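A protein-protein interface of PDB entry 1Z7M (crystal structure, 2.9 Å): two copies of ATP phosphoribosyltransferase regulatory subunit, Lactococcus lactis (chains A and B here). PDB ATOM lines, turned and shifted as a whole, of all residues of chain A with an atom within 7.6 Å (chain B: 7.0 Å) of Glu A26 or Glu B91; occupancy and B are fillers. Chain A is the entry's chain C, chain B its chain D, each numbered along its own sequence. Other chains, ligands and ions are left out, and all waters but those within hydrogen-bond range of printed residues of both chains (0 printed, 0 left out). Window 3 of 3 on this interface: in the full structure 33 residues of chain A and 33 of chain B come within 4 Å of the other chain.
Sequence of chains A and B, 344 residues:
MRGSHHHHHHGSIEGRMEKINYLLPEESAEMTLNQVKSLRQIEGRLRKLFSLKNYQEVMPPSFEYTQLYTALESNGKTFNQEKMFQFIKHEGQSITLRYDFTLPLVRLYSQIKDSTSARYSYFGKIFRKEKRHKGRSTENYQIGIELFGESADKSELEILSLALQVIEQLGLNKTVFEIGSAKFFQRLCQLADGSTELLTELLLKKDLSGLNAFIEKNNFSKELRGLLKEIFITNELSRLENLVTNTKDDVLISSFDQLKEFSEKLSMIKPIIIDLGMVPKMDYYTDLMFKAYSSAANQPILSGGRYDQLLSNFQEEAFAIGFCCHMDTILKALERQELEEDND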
ATOM      1  N   LEU A  23      12.754  -1.855 -22.791  1.00  0.00           N
ATOM      2  CA  LEU A  23      11.498  -1.638 -23.503  1.00  0.00           C
ATOM      3  C   LEU A  23      11.710  -1.368 -24.990  1.00  0.00           C
ATOM      4  O   LEU A  23      12.836  -1.200 -25.451  1.00  0.00           O
ATOM      5  CB  LEU A  23      10.729  -0.470 -22.874  1.00  0.00           C
ATOM      6  CG  LEU A  23       9.916  -0.717 -21.597  1.00  0.00           C
ATOM      7  CD1 LEU A  23       9.422   0.627 -21.030  1.00  0.00           C
ATOM      8  CD2 LEU A  23       8.741  -1.652 -21.905  1.00  0.00           C
ATOM      9  N   LEU A  24      10.612  -1.331 -25.734  1.00  0.00           N
ATOM     10  CA  LEU A  24      10.664  -1.093 -27.166  1.00  0.00           C
ATOM     11  C   LEU A  24       9.420  -0.340 -27.633  1.00  0.00           C
ATOM     12  O   LEU A  24       8.318  -0.564 -27.126  1.00  0.00           O
ATOM     13  CB  LEU A  24      10.739  -2.423 -27.920  1.00  0.00           C
ATOM     14  CG  LEU A  24      11.943  -2.721 -28.816  1.00  0.00           C
ATOM     15  CD1 LEU A  24      13.134  -3.122 -27.938  1.00  0.00           C
ATOM     16  CD2 LEU A  24      11.584  -3.842 -29.807  1.00  0.00           C
ATOM     17  N   PRO A  25       9.582   0.556 -28.618  1.00  0.00           N
ATOM     18  CA  PRO A  25       8.449   1.321 -29.137  1.00  0.00           C
ATOM     19  C   PRO A  25       7.316   0.387 -29.536  1.00  0.00           C
ATOM     20  O   PRO A  25       7.541  -0.674 -30.116  1.00  0.00           O
ATOM     21  CB  PRO A  25       9.046   2.047 -30.339  1.00  0.00           C
ATOM     22  CG  PRO A  25      10.446   2.276 -29.917  1.00  0.00           C
ATOM     23  CD  PRO A  25      10.830   0.955 -29.293  1.00  0.00           C
ATOM     24  N   GLU A  26       6.100   0.789 -29.207  1.00  0.00           N
ATOM     25  CA  GLU A  26       4.935   0.005 -29.533  1.00  0.00           C
ATOM     26  C   GLU A  26       4.842  -0.101 -31.053  1.00  0.00           C
ATOM     27  O   GLU A  26       4.091  -0.914 -31.576  1.00  0.00           O
ATOM     28  CB  GLU A  26       3.690   0.683 -28.949  1.00  0.00           C
ATOM     29  CG  GLU A  26       3.756   0.886 -27.424  1.00  0.00           C
ATOM     30  CD  GLU A  26       3.056   2.161 -26.936  1.00  0.00           C
ATOM     31  OE1 GLU A  26       3.022   2.389 -25.704  1.00  0.00           O
ATOM     32  OE2 GLU A  26       2.546   2.937 -27.780  1.00  0.00           O
ATOM     33  N   GLU A  27       5.625   0.707 -31.763  1.00  0.00           N
ATOM     34  CA  GLU A  27       5.610   0.695 -33.230  1.00  0.00           C
ATOM     35  C   GLU A  27       6.771  -0.101 -33.843  1.00  0.00           C
ATOM     36  O   GLU A  27       6.680  -0.581 -34.980  1.00  0.00           O
ATOM     37  CB  GLU A  27       5.616   2.135 -33.757  1.00  0.00           C
ATOM     38  CG  GLU A  27       4.410   2.939 -33.295  1.00  0.00           C
ATOM     39  CD  GLU A  27       4.785   4.138 -32.445  1.00  0.00           C
ATOM     40  OE1 GLU A  27       5.625   3.979 -31.526  1.00  0.00           O
ATOM     41  OE2 GLU A  27       4.227   5.237 -32.687  1.00  0.00           O
ATOM     42  N   SER A  28       7.852  -0.243 -33.079  1.00  0.00           N
ATOM     43  CA  SER A  28       9.020  -0.983 -33.533  1.00  0.00           C
ATOM     44  C   SER A  28       8.659  -2.454 -33.542  1.00  0.00           C
ATOM     45  O   SER A  28       8.146  -2.978 -32.552  1.00  0.00           O
ATOM     46  CB  SER A  28      10.210  -0.773 -32.585  1.00  0.00           C
ATOM     47  OG  SER A  28      10.140  -1.632 -31.450  1.00  0.00           O
ATOM     48  N   ALA A  29       8.924  -3.112 -34.666  1.00  0.00           N
ATOM     49  CA  ALA A  29       8.647  -4.535 -34.803  1.00  0.00           C
ATOM     50  C   ALA A  29       9.953  -5.311 -34.681  1.00  0.00           C
ATOM     51  O   ALA A  29      11.039  -4.773 -34.904  1.00  0.00           O
ATOM     52  CB  ALA A  29       7.996  -4.815 -36.137  1.00  0.00           C
ATOM     53  N   GLU A 130      -0.242   2.284 -35.291  1.00  0.00           N
ATOM     54  CA  GLU A 130      -1.260   1.332 -34.871  1.00  0.00           C
ATOM     55  C   GLU A 130      -1.569   1.408 -33.370  1.00  0.00           C
ATOM     56  O   GLU A 130      -0.855   2.063 -32.602  1.00  0.00           O
ATOM     57  CB  GLU A 130      -0.795  -0.076 -35.247  1.00  0.00           C
ATOM     58  CG  GLU A 130      -1.839  -0.912 -35.951  1.00  0.00           C
ATOM     59  CD  GLU A 130      -2.600  -0.129 -37.004  1.00  0.00           C
ATOM     60  OE1 GLU A 130      -1.987   0.302 -38.009  1.00  0.00           O
ATOM     61  OE2 GLU A 130      -3.823   0.059 -36.817  1.00  0.00           O
ATOM     62  N   TYR B  65      13.370   3.948 -29.059  1.00  0.00           N
ATOM     63  CA  TYR B  65      13.146   5.030 -28.101  1.00  0.00           C
ATOM     64  C   TYR B  65      14.380   5.902 -28.200  1.00  0.00           C
ATOM     65  O   TYR B  65      15.497   5.399 -28.076  1.00  0.00           O
ATOM     66  CB  TYR B  65      13.028   4.494 -26.674  1.00  0.00           C
ATOM     67  CG  TYR B  65      11.648   4.011 -26.328  1.00  0.00           C
ATOM     68  CD1 TYR B  65      11.435   2.713 -25.870  1.00  0.00           C
ATOM     69  CD2 TYR B  65      10.544   4.843 -26.488  1.00  0.00           C
ATOM     70  CE1 TYR B  65      10.147   2.250 -25.588  1.00  0.00           C
ATOM     71  CE2 TYR B  65       9.255   4.397 -26.210  1.00  0.00           C
ATOM     72  CZ  TYR B  65       9.059   3.102 -25.765  1.00  0.00           C
ATOM     73  OH  TYR B  65       7.775   2.659 -25.530  1.00  0.00           O
ATOM     74  N   ILE B  88       6.652  12.016 -31.622  1.00  0.00           N
ATOM     75  CA  ILE B  88       6.062  11.485 -30.426  1.00  0.00           C
ATOM     76  C   ILE B  88       5.123  10.328 -30.736  1.00  0.00           C
ATOM     77  O   ILE B  88       4.334  10.392 -31.679  1.00  0.00           O
ATOM     78  CB  ILE B  88       5.315  12.598 -29.672  1.00  0.00           C
ATOM     79  CG1 ILE B  88       6.194  13.844 -29.573  1.00  0.00           C
ATOM     80  CG2 ILE B  88       4.934  12.116 -28.284  1.00  0.00           C
ATOM     81  CD1 ILE B  88       7.504  13.667 -28.829  1.00  0.00           C
ATOM     82  N   LYS B  89       5.240   9.261 -29.944  1.00  0.00           N
ATOM     83  CA  LYS B  89       4.399   8.078 -30.093  1.00  0.00           C
ATOM     84  C   LYS B  89       3.146   8.321 -29.267  1.00  0.00           C
ATOM     85  O   LYS B  89       3.130   9.188 -28.390  1.00  0.00           O
ATOM     86  CB  LYS B  89       5.123   6.835 -29.588  1.00  0.00           C
ATOM     87  CG  LYS B  89       5.412   6.822 -28.102  1.00  0.00           C
ATOM     88  CD  LYS B  89       6.295   5.628 -27.743  1.00  0.00           C
ATOM     89  CE  LYS B  89       5.641   4.663 -26.731  1.00  0.00           C
ATOM     90  NZ  LYS B  89       5.683   5.111 -25.298  1.00  0.00           N
ATOM     91  N   HIS B  90       2.097   7.555 -29.542  1.00  0.00           N
ATOM     92  CA  HIS B  90       0.838   7.728 -28.842  1.00  0.00           C
ATOM     93  C   HIS B  90       1.005   7.810 -27.327  1.00  0.00           C
ATOM     94  O   HIS B  90       0.430   8.686 -26.672  1.00  0.00           O
ATOM     95  CB  HIS B  90      -0.118   6.579 -29.168  1.00  0.00           C
ATOM     96  N   GLU B  91       1.818   6.918 -26.775  1.00  0.00           N
ATOM     97  CA  GLU B  91       2.054   6.891 -25.340  1.00  0.00           C
ATOM     98  C   GLU B  91       2.675   8.199 -24.859  1.00  0.00           C
ATOM     99  O   GLU B  91       2.720   8.464 -23.660  1.00  0.00           O
ATOM    100  CB  GLU B  91       2.965   5.713 -24.996  1.00  0.00           C
ATOM    101  CG  GLU B  91       2.784   5.159 -23.592  1.00  0.00           C
ATOM    102  CD  GLU B  91       1.363   4.663 -23.340  1.00  0.00           C
ATOM    103  OE1 GLU B  91       0.420   5.491 -23.367  1.00  0.00           O
ATOM    104  OE2 GLU B  91       1.191   3.446 -23.100  1.00  0.00           O
ATOM    105  N   GLY B  92       3.163   9.005 -25.801  1.00  0.00           N
ATOM    106  CA  GLY B  92       3.755  10.289 -25.457  1.00  0.00           C
ATOM    107  C   GLY B  92       5.273  10.381 -25.425  1.00  0.00           C
ATOM    108  O   GLY B  92       5.817  11.462 -25.224  1.00  0.00           O
ATOM    109  N   GLN B  93       5.955   9.255 -25.618  1.00  0.00           N
ATOM    110  CA  GLN B  93       7.425   9.184 -25.611  1.00  0.00           C
ATOM    111  C   GLN B  93       8.059   9.688 -26.917  1.00  0.00           C
ATOM    112  O   GLN B  93       7.369   9.881 -27.913  1.00  0.00           O
ATOM    113  CB  GLN B  93       7.860   7.736 -25.391  1.00  0.00           C
ATOM    114  CG  GLN B  93       7.536   7.159 -24.033  1.00  0.00           C
ATOM    115  CD  GLN B  93       8.615   7.464 -23.018  1.00  0.00           C
ATOM    116  OE1 GLN B  93       8.835   8.626 -22.659  1.00  0.00           O
ATOM    117  NE2 GLN B  93       9.311   6.417 -22.557  1.00  0.00           N
ATOM    118  N   ILE B  95      10.317   8.847 -29.983  1.00  0.00           N
ATOM    119  CA  ILE B  95      10.932   7.764 -30.723  1.00  0.00           C
ATOM    120  C   ILE B  95      11.751   8.346 -31.863  1.00  0.00           C
ATOM    121  O   ILE B  95      11.528   9.481 -32.282  1.00  0.00           O
ATOM    122  CB  ILE B  95       9.866   6.784 -31.277  1.00  0.00           C
ATOM    123  CG1 ILE B  95       8.848   7.533 -32.129  1.00  0.00           C
ATOM    124  CG2 ILE B  95       9.157   6.074 -30.122  1.00  0.00           C
ATOM    125  CD1 ILE B  95       7.785   6.642 -32.727  1.00  0.00           C
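The side-chain hydroxyl (OH) of Tyr B65 sits close to the side-chain amino group (NZ) of Lys B89 (3.2 Å). The backbone carbonyl oxygen (O) of Pro A25 lies within hydrogen-bond range of the side-chain hydroxyl (OG) of Ser A28 (3.1 Å).
Glu A26 touches two residues of chain B. Of chain A, only Glu A26 comes within 4 Å of Glu B91. No residue of chain A comes within 4 Å of His B90. Printed residues of chain B within 4 Å of Leu A23: Tyr B65 (3.9 Å). Printed residues of chain B within 4 Å of Leu A24: Tyr B65 (3.4 Å). Of the printed residues of chain B, Pro A25 touches Tyr B65 (3.5 Å). Ser A28 touches none of the printed residues of chain B. Ala A29 touches none of the printed residues of chain B. The nearest residue of chain A that does not touch Glu B91 is Glu A27 (6.6 Å). The nearest printed residue of chain B that does not touch Leu A24 is Lys B89 (5.9 Å).
The side-chain carboxylate (OE1) of Glu A26 sits close to the side-chain carboxylate (OE2) of Glu B91, at 3.4 Å. The side-chain carboxylate of Glu A26 lies within salt-bridge range of the side-chain amino group of Lys B89 (3.8 Å).
No position is printed for both chains. Of the 7 pairs that touch across the chains among the printed residues, none has its exchanged pair printed and touching as well.
Among the printed residues, merely in contact across the chains: Leu A23 with Tyr B65 (3.9 Å), Leu A24 with Tyr B65 (3.4 Å), Pro A25 with Tyr B65 (3.5 Å), Glu A27 with Lys B89 (3.5 Å) and Glu A27 with Ile B95 (3.6 Å).
Of the 8 printed residues of chain A, 5 touch a printed residue of chain B. Hydrophobic or aromatic side chains of chain A within 4 Å of the printed part of chain B: Leu A23 and Pro A25. Along chain A the printed residues that touch a printed residue of chain B span positions 23 to 27. Among the printed residues, Asp or Glu carboxylates within 4 Å of a Lys or Arg side-chain nitrogen of the other chain: Glu A26 with Lys B89 (3.8 Å).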
